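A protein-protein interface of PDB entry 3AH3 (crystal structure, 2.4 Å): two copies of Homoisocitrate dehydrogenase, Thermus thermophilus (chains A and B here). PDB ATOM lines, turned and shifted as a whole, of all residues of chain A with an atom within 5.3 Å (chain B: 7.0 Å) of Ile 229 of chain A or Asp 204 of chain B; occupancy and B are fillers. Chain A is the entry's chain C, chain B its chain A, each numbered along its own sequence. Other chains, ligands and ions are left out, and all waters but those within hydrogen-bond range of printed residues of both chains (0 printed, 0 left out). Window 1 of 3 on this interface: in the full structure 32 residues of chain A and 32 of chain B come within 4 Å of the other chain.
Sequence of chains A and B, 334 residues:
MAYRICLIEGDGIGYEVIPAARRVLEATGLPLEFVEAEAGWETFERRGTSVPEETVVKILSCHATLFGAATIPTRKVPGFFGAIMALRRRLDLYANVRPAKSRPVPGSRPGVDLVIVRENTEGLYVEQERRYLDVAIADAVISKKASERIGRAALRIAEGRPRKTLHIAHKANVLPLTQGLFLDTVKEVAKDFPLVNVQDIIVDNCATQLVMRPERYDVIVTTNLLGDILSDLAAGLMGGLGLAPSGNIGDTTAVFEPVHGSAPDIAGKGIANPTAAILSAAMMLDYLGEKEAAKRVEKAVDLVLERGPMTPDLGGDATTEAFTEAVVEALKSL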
ATOM      1  N   LEU A 225       4.916 -17.537  15.925  1.00  0.00           N
ATOM      2  CA  LEU A 225       4.143 -18.581  16.644  1.00  0.00           C
ATOM      3  C   LEU A 225       4.945 -19.043  17.857  1.00  0.00           C
ATOM      4  O   LEU A 225       4.397 -19.527  18.856  1.00  0.00           O
ATOM      5  CB  LEU A 225       3.790 -19.790  15.748  1.00  0.00           C
ATOM      6  CG  LEU A 225       4.722 -21.020  15.636  1.00  0.00           C
ATOM      7  CD1 LEU A 225       4.581 -22.007  16.806  1.00  0.00           C
ATOM      8  CD2 LEU A 225       4.463 -21.735  14.318  1.00  0.00           C
ATOM      9  N   LEU A 226       6.257 -18.868  17.734  1.00  0.00           N
ATOM     10  CA  LEU A 226       7.237 -19.503  18.584  1.00  0.00           C
ATOM     11  C   LEU A 226       7.749 -18.536  19.644  1.00  0.00           C
ATOM     12  O   LEU A 226       7.867 -18.891  20.825  1.00  0.00           O
ATOM     13  CB  LEU A 226       8.384 -19.988  17.701  1.00  0.00           C
ATOM     14  CG  LEU A 226       9.234 -21.150  18.188  1.00  0.00           C
ATOM     15  CD1 LEU A 226      10.019 -21.773  17.029  1.00  0.00           C
ATOM     16  CD2 LEU A 226      10.155 -20.627  19.262  1.00  0.00           C
ATOM     17  N   GLY A 227       8.049 -17.313  19.219  1.00  0.00           N
ATOM     18  CA  GLY A 227       8.474 -16.277  20.143  1.00  0.00           C
ATOM     19  C   GLY A 227       7.373 -16.058  21.150  1.00  0.00           C
ATOM     20  O   GLY A 227       7.632 -15.936  22.350  1.00  0.00           O
ATOM     21  N   ASP A 228       6.141 -16.034  20.639  1.00  0.00           N
ATOM     22  CA  ASP A 228       4.970 -15.716  21.436  1.00  0.00           C
ATOM     23  C   ASP A 228       4.811 -16.722  22.560  1.00  0.00           C
ATOM     24  O   ASP A 228       4.727 -16.346  23.724  1.00  0.00           O
ATOM     25  CB  ASP A 228       3.738 -15.632  20.540  1.00  0.00           C
ATOM     26  CG  ASP A 228       3.779 -14.410  19.612  1.00  0.00           C
ATOM     27  OD1 ASP A 228       4.512 -13.432  19.932  1.00  0.00           O
ATOM     28  OD2 ASP A 228       3.088 -14.431  18.562  1.00  0.00           O
ATOM     29  N   ILE A 229       4.839 -17.999  22.202  1.00  0.00           N
ATOM     30  CA  ILE A 229       4.773 -19.067  23.175  1.00  0.00           C
ATOM     31  C   ILE A 229       5.911 -18.958  24.223  1.00  0.00           C
ATOM     32  O   ILE A 229       5.647 -19.032  25.421  1.00  0.00           O
ATOM     33  CB  ILE A 229       4.610 -20.470  22.459  1.00  0.00           C
ATOM     34  CG1 ILE A 229       3.523 -21.331  23.132  1.00  0.00           C
ATOM     35  CG2 ILE A 229       5.944 -21.180  22.206  1.00  0.00           C
ATOM     36  CD1 ILE A 229       3.839 -21.803  24.517  1.00  0.00           C
ATOM     37  N   LEU A 230       7.143 -18.713  23.784  1.00  0.00           N
ATOM     38  CA  LEU A 230       8.270 -18.490  24.712  1.00  0.00           C
ATOM     39  C   LEU A 230       8.091 -17.237  25.579  1.00  0.00           C
ATOM     40  O   LEU A 230       8.399 -17.247  26.770  1.00  0.00           O
ATOM     41  CB  LEU A 230       9.605 -18.407  23.963  1.00  0.00           C
ATOM     42  CG  LEU A 230      10.130 -19.613  23.177  1.00  0.00           C
ATOM     43  CD1 LEU A 230      11.329 -19.204  22.379  1.00  0.00           C
ATOM     44  CD2 LEU A 230      10.484 -20.781  24.075  1.00  0.00           C
ATOM     45  N   SER A 231       7.595 -16.162  24.968  1.00  0.00           N
ATOM     46  CA  SER A 231       7.308 -14.914  25.674  1.00  0.00           C
ATOM     47  C   SER A 231       6.191 -15.082  26.689  1.00  0.00           C
ATOM     48  O   SER A 231       6.205 -14.435  27.738  1.00  0.00           O
ATOM     49  CB  SER A 231       6.932 -13.805  24.688  1.00  0.00           C
ATOM     50  OG  SER A 231       8.079 -13.183  24.144  1.00  0.00           O
ATOM     51  N   ASP A 232       5.227 -15.944  26.376  1.00  0.00           N
ATOM     52  CA  ASP A 232       4.085 -16.178  27.259  1.00  0.00           C
ATOM     53  C   ASP A 232       4.472 -16.985  28.484  1.00  0.00           C
ATOM     54  O   ASP A 232       3.927 -16.800  29.568  1.00  0.00           O
ATOM     55  CB  ASP A 232       2.958 -16.880  26.505  1.00  0.00           C
ATOM     56  CG  ASP A 232       2.281 -15.971  25.508  1.00  0.00           C
ATOM     57  OD1 ASP A 232       1.813 -14.880  25.902  1.00  0.00           O
ATOM     58  OD2 ASP A 232       2.225 -16.352  24.321  1.00  0.00           O
ATOM     59  N   LEU A 233       5.412 -17.894  28.280  1.00  0.00           N
ATOM     60  CA  LEU A 233       5.985 -18.690  29.336  1.00  0.00           C
ATOM     61  C   LEU A 233       6.846 -17.775  30.219  1.00  0.00           C
ATOM     62  O   LEU A 233       6.783 -17.839  31.450  1.00  0.00           O
ATOM     63  CB  LEU A 233       6.820 -19.796  28.682  1.00  0.00           C
ATOM     64  CG  LEU A 233       7.593 -20.837  29.482  1.00  0.00           C
ATOM     65  CD1 LEU A 233       8.135 -21.858  28.499  1.00  0.00           C
ATOM     66  CD2 LEU A 233       8.724 -20.200  30.281  1.00  0.00           C
ATOM     67  N   ALA A 234       7.636 -16.921  29.573  1.00  0.00           N
ATOM     68  CA  ALA A 234       8.467 -15.942  30.256  1.00  0.00           C
ATOM     69  C   ALA A 234       7.625 -15.023  31.121  1.00  0.00           C
ATOM     70  O   ALA A 234       7.981 -14.763  32.271  1.00  0.00           O
ATOM     71  CB  ALA A 234       9.268 -15.133  29.252  1.00  0.00           C
ATOM     72  N   ALA B 169      -6.213 -26.640  23.976  1.00  0.00           N
ATOM     73  CA  ALA B 169      -5.294 -25.520  23.758  1.00  0.00           C
ATOM     74  C   ALA B 169      -5.037 -25.340  22.269  1.00  0.00           C
ATOM     75  O   ALA B 169      -4.555 -26.256  21.585  1.00  0.00           O
ATOM     76  CB  ALA B 169      -3.996 -25.741  24.505  1.00  0.00           C
ATOM     77  N   HIS B 170      -5.363 -24.151  21.773  1.00  0.00           N
ATOM     78  CA  HIS B 170      -5.453 -23.920  20.333  1.00  0.00           C
ATOM     79  C   HIS B 170      -4.977 -22.508  19.955  1.00  0.00           C
ATOM     80  O   HIS B 170      -4.728 -21.676  20.833  1.00  0.00           O
ATOM     81  CB  HIS B 170      -6.911 -24.092  19.913  1.00  0.00           C
ATOM     82  CG  HIS B 170      -7.801 -23.006  20.432  1.00  0.00           C
ATOM     83  ND1 HIS B 170      -8.402 -23.061  21.674  1.00  0.00           N
ATOM     84  CD2 HIS B 170      -8.149 -21.813  19.900  1.00  0.00           C
ATOM     85  CE1 HIS B 170      -9.101 -21.957  21.871  1.00  0.00           C
ATOM     86  NE2 HIS B 170      -8.966 -21.185  20.808  1.00  0.00           N
ATOM     87  N   LYS B 171      -4.893 -22.239  18.653  1.00  0.00           N
ATOM     88  CA  LYS B 171      -4.584 -20.899  18.136  1.00  0.00           C
ATOM     89  C   LYS B 171      -5.647 -20.389  17.154  1.00  0.00           C
ATOM     90  O   LYS B 171      -5.324 -19.714  16.178  1.00  0.00           O
ATOM     91  CB  LYS B 171      -3.217 -20.886  17.450  1.00  0.00           C
ATOM     92  CG  LYS B 171      -2.061 -20.541  18.347  1.00  0.00           C
ATOM     93  CD  LYS B 171      -0.859 -20.135  17.498  1.00  0.00           C
ATOM     94  CE  LYS B 171       0.124 -19.299  18.270  1.00  0.00           C
ATOM     95  NZ  LYS B 171      -0.293 -17.884  18.274  1.00  0.00           N
ATOM     96  N   ASN B 173      -7.679 -18.052  17.324  1.00  0.00           N
ATOM     97  CA  ASN B 173      -7.734 -16.590  17.268  1.00  0.00           C
ATOM     98  C   ASN B 173      -6.932 -15.975  16.115  1.00  0.00           C
ATOM     99  O   ASN B 173      -7.248 -14.866  15.655  1.00  0.00           O
ATOM    100  CB  ASN B 173      -7.308 -15.965  18.604  1.00  0.00           C
ATOM    101  CG  ASN B 173      -5.885 -16.335  19.005  1.00  0.00           C
ATOM    102  OD1 ASN B 173      -5.440 -17.465  18.806  1.00  0.00           O
ATOM    103  ND2 ASN B 173      -5.172 -15.382  19.583  1.00  0.00           N
ATOM    104  N   VAL B 174      -5.894 -16.684  15.666  1.00  0.00           N
ATOM    105  CA  VAL B 174      -5.025 -16.212  14.580  1.00  0.00           C
ATOM    106  C   VAL B 174      -4.942 -17.196  13.403  1.00  0.00           C
ATOM    107  O   VAL B 174      -4.588 -16.804  12.291  1.00  0.00           O
ATOM    108  CB  VAL B 174      -3.586 -15.850  15.074  1.00  0.00           C
ATOM    109  CG1 VAL B 174      -3.638 -14.727  16.106  1.00  0.00           C
ATOM    110  CG2 VAL B 174      -2.856 -17.072  15.632  1.00  0.00           C
ATOM    111  N   ILE B 201      -8.973 -22.960  25.491  1.00  0.00           N
ATOM    112  CA  ILE B 201      -8.023 -21.923  25.881  1.00  0.00           C
ATOM    113  C   ILE B 201      -6.999 -21.674  24.770  1.00  0.00           C
ATOM    114  O   ILE B 201      -6.472 -22.613  24.168  1.00  0.00           O
ATOM    115  CB  ILE B 201      -7.318 -22.282  27.232  1.00  0.00           C
ATOM    116  CG1 ILE B 201      -6.496 -21.104  27.762  1.00  0.00           C
ATOM    117  CG2 ILE B 201      -6.466 -23.562  27.110  1.00  0.00           C
ATOM    118  CD1 ILE B 201      -6.014 -21.289  29.184  1.00  0.00           C
ATOM    119  N   ILE B 202      -6.741 -20.398  24.499  1.00  0.00           N
ATOM    120  CA  ILE B 202      -5.638 -19.974  23.626  1.00  0.00           C
ATOM    121  C   ILE B 202      -4.326 -20.528  24.195  1.00  0.00           C
ATOM    122  O   ILE B 202      -4.004 -20.300  25.365  1.00  0.00           O
ATOM    123  CB  ILE B 202      -5.576 -18.415  23.506  1.00  0.00           C
ATOM    124  CG1 ILE B 202      -6.965 -17.816  23.208  1.00  0.00           C
ATOM    125  CG2 ILE B 202      -4.519 -17.963  22.489  1.00  0.00           C
ATOM    126  CD1 ILE B 202      -7.615 -18.297  21.920  1.00  0.00           C
ATOM    127  N   VAL B 203      -3.588 -21.270  23.367  1.00  0.00           N
ATOM    128  CA  VAL B 203      -2.371 -21.954  23.809  1.00  0.00           C
ATOM    129  C   VAL B 203      -1.410 -21.006  24.547  1.00  0.00           C
ATOM    130  O   VAL B 203      -0.754 -21.398  25.512  1.00  0.00           O
ATOM    131  CB  VAL B 203      -1.661 -22.709  22.640  1.00  0.00           C
ATOM    132  CG1 VAL B 203      -1.068 -21.744  21.615  1.00  0.00           C
ATOM    133  CG2 VAL B 203      -0.587 -23.654  23.181  1.00  0.00           C
ATOM    134  N   ASP B 204      -1.365 -19.753  24.103  1.00  0.00           N
ATOM    135  CA  ASP B 204      -0.490 -18.747  24.692  1.00  0.00           C
ATOM    136  C   ASP B 204      -0.814 -18.497  26.152  1.00  0.00           C
ATOM    137  O   ASP B 204       0.091 -18.511  26.997  1.00  0.00           O
ATOM    138  CB  ASP B 204      -0.578 -17.455  23.890  1.00  0.00           C
ATOM    139  CG  ASP B 204      -0.096 -17.637  22.469  1.00  0.00           C
ATOM    140  OD1 ASP B 204       1.134 -17.782  22.282  1.00  0.00           O
ATOM    141  OD2 ASP B 204      -0.948 -17.662  21.547  1.00  0.00           O
ATOM    142  N   ASN B 205      -2.095 -18.262  26.440  1.00  0.00           N
ATOM    143  CA  ASN B 205      -2.583 -18.121  27.812  1.00  0.00           C
ATOM    144  C   ASN B 205      -2.382 -19.407  28.595  1.00  0.00           C
ATOM    145  O   ASN B 205      -2.170 -19.384  29.805  1.00  0.00           O
ATOM    146  CB  ASN B 205      -4.067 -17.746  27.831  1.00  0.00           C
ATOM    147  CG  ASN B 205      -4.331 -16.385  27.242  1.00  0.00           C
ATOM    148  OD1 ASN B 205      -3.462 -15.516  27.250  1.00  0.00           O
ATOM    149  ND2 ASN B 205      -5.537 -16.189  26.722  1.00  0.00           N
ATOM    150  N   CYS B 206      -2.462 -20.535  27.897  1.00  0.00           N
ATOM    151  CA  CYS B 206      -2.285 -21.833  28.545  1.00  0.00           C
ATOM    152  C   CYS B 206      -0.876 -21.938  29.112  1.00  0.00           C
ATOM    153  O   CYS B 206      -0.696 -22.332  30.267  1.00  0.00           O
ATOM    154  CB  CYS B 206      -2.587 -22.988  27.584  1.00  0.00           C
ATOM    155  SG  CYS B 206      -2.543 -24.630  28.348  1.00  0.00           S
ATOM    156  N   ALA B 207       0.109 -21.552  28.304  1.00  0.00           N
ATOM    157  CA  ALA B 207       1.519 -21.532  28.706  1.00  0.00           C
ATOM    158  C   ALA B 207       1.791 -20.653  29.927  1.00  0.00           C
ATOM    159  O   ALA B 207       2.503 -21.070  30.840  1.00  0.00           O
ATOM    160  CB  ALA B 207       2.391 -21.095  27.543  1.00  0.00           C
ATOM    161  N   THR B 208       1.226 -19.444  29.947  1.00  0.00           N
ATOM    162  CA  THR B 208       1.412 -18.546  31.091  1.00  0.00           C
ATOM    163  C   THR B 208       0.873 -19.217  32.349  1.00  0.00           C
ATOM    164  O   THR B 208       1.539 -19.244  33.388  1.00  0.00           O
ATOM    165  CB  THR B 208       0.744 -17.157  30.886  1.00  0.00           C
ATOM    166  OG1 THR B 208       1.103 -16.627  29.609  1.00  0.00           O
ATOM    167  CG2 THR B 208       1.210 -16.178  31.935  1.00  0.00           C
ATOM    168  N   GLN B 209      -0.321 -19.791  32.221  1.00  0.00           N
ATOM    169  CA  GLN B 209      -0.988 -20.472  33.318  1.00  0.00           C
ATOM    170  C   GLN B 209      -0.259 -21.717  33.796  1.00  0.00           C
ATOM    171  O   GLN B 209      -0.171 -21.946  35.001  1.00  0.00           O
ATOM    172  CB  GLN B 209      -2.434 -20.797  32.949  1.00  0.00           C
ATOM    173  CG  GLN B 209      -3.307 -19.564  32.823  1.00  0.00           C
ATOM    174  CD  GLN B 209      -3.059 -18.591  33.940  1.00  0.00           C
ATOM    175  OE1 GLN B 209      -3.244 -18.912  35.115  1.00  0.00           O
ATOM    176  NE2 GLN B 209      -2.609 -17.398  33.588  1.00  0.00           N
ATOM    177  N   LEU B 225       3.508 -29.819  17.820  1.00  0.00           N
ATOM    178  CA  LEU B 225       4.426 -28.668  17.859  1.00  0.00           C
ATOM    179  C   LEU B 225       4.054 -27.761  19.034  1.00  0.00           C
ATOM    180  O   LEU B 225       4.939 -27.242  19.727  1.00  0.00           O
ATOM    181  CB  LEU B 225       4.461 -27.885  16.531  1.00  0.00           C
ATOM    182  CG  LEU B 225       5.618 -28.073  15.529  1.00  0.00           C
ATOM    183  CD1 LEU B 225       5.721 -29.490  14.941  1.00  0.00           C
ATOM    184  CD2 LEU B 225       5.500 -27.051  14.404  1.00  0.00           C
ATOM    185  N   LEU B 226       2.746 -27.589  19.252  1.00  0.00           N
ATOM    186  CA  LEU B 226       2.241 -26.880  20.430  1.00  0.00           C
ATOM    187  C   LEU B 226       2.348 -27.737  21.687  1.00  0.00           C
ATOM    188  O   LEU B 226       2.863 -27.292  22.719  1.00  0.00           O
ATOM    189  CB  LEU B 226       0.792 -26.416  20.223  1.00  0.00           C
ATOM    190  CG  LEU B 226       0.511 -24.945  19.860  1.00  0.00           C
ATOM    191  CD1 LEU B 226       1.731 -24.156  19.290  1.00  0.00           C
ATOM    192  CD2 LEU B 226      -0.692 -24.853  18.937  1.00  0.00           C
ATOM    193  N   ILE B 229       6.074 -28.073  23.021  1.00  0.00           N
ATOM    194  CA  ILE B 229       6.478 -26.935  23.814  1.00  0.00           C
ATOM    195  C   ILE B 229       5.771 -26.925  25.183  1.00  0.00           C
ATOM    196  O   ILE B 229       6.397 -26.605  26.193  1.00  0.00           O
ATOM    197  CB  ILE B 229       6.421 -25.592  23.002  1.00  0.00           C
ATOM    198  CG1 ILE B 229       7.323 -24.521  23.627  1.00  0.00           C
ATOM    199  CG2 ILE B 229       5.004 -25.092  22.814  1.00  0.00           C
ATOM    200  CD1 ILE B 229       6.754 -23.843  24.884  1.00  0.00           C
ATOM    201  N   LEU B 230       4.502 -27.321  25.230  1.00  0.00           N
ATOM    202  CA  LEU B 230       3.777 -27.388  26.515  1.00  0.00           C
ATOM    203  C   LEU B 230       4.315 -28.478  27.452  1.00  0.00           C
ATOM    204  O   LEU B 230       4.336 -28.300  28.674  1.00  0.00           O
ATOM    205  CB  LEU B 230       2.265 -27.553  26.321  1.00  0.00           C
ATOM    206  CG  LEU B 230       1.430 -26.410  25.741  1.00  0.00           C
ATOM    207  CD1 LEU B 230      -0.058 -26.749  25.846  1.00  0.00           C
ATOM    208  CD2 LEU B 230       1.714 -25.086  26.422  1.00  0.00           C
ATOM    209  N   LEU B 233       7.762 -27.027  28.807  1.00  0.00           N
ATOM    210  CA  LEU B 233       7.433 -26.162  29.926  1.00  0.00           C
ATOM    211  C   LEU B 233       7.140 -27.015  31.163  1.00  0.00           C
ATOM    212  O   LEU B 233       7.778 -26.850  32.202  1.00  0.00           O
ATOM    213  CB  LEU B 233       6.223 -25.281  29.564  1.00  0.00           C
ATOM    214  CG  LEU B 233       5.738 -24.186  30.521  1.00  0.00           C
ATOM    215  CD1 LEU B 233       4.715 -23.291  29.832  1.00  0.00           C
ATOM    216  CD2 LEU B 233       5.145 -24.764  31.805  1.00  0.00           C
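The side-chain carboxylate (OD1) of Asp 204 of chain B sits close to the side-chain carboxylate (OD2) of Asp 232 of chain A, 2.7 Å away.
OG1 of Thr 208 of chain B lies within hydrogen-bond range of O of Asp 232 of chain A (2.8 Å).
OD2 of Asp 204 of chain B lies within salt-bridge range of NZ of Lys 171 of chain B, 3.3 Å away.
The backbone carbonyl oxygen of Asp 204 of chain B lies within hydrogen-bond range of the side-chain hydroxyl of Thr 208 of chain B (3.4 Å).
O of Asp 228 of chain A sits close to OD2 of Asp 232 of chain A (2.6 Å).
CB of Asp 228 of chain A touches OD1 of Asp 204 of chain B, at 3.8 Å.
Asp 204 of chain B touches Ile 229 of chain A (OD1 to N, 3.7 Å).
Ile 229 of chain A touches Ala 207 of chain B.
Ile 229 of chain A touches Ile 229 of chain B (CD1 to CD1, 3.6 Å).
Leu 233 of chain B touches Leu 233 of chain A (CD1 to CG, 3.8 Å).
Printed residues of chain B within 4 Å of Asp 228 of chain A: Asp 204.
Ile 229 of chain A touches just these residues of chain B: Asp 204 (3.7 Å), Ala 207 (3.4 Å) and Ile 229 (3.6 Å).
Of the printed residues of chain B, Asp 232 of chain A touches Asp 204 (2.7 Å) and Thr 208 (2.8 Å).
Printed residues of chain A within 4 Å of Asp 204 of chain B: Asp 228 (3.8 Å), Ile 229 (3.7 Å) and Asp 232 (2.7 Å).
Of the printed residues of chain A, Ala 207 of chain B touches Ile 229 (3.4 Å).
Of the printed residues of chain A, Thr 208 of chain B touches Asp 232 (2.8 Å).
Hydrophobic or aromatic side chains of chain A within 4 Å of the printed part of chain B: Ile 229 and Leu 233.
Of the 19 printed residues of chain B, 5 touch a printed residue of chain A.
Among the printed residues, 7 pairs touch across the chains.
Among the printed residues, no Asp or Glu carboxylate lies within 4 Å of a Lys or Arg side-chain nitrogen of the other chain.
Ile 229 of chain A touches its own counterpart, Ile 229 of chain B.
Leu 233 of chain B touches its own counterpart, Leu 233 of chain A.
Of the 7 pairs that touch across the chains among the printed residues, 2 have their exchanged pair printed and touching as well.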
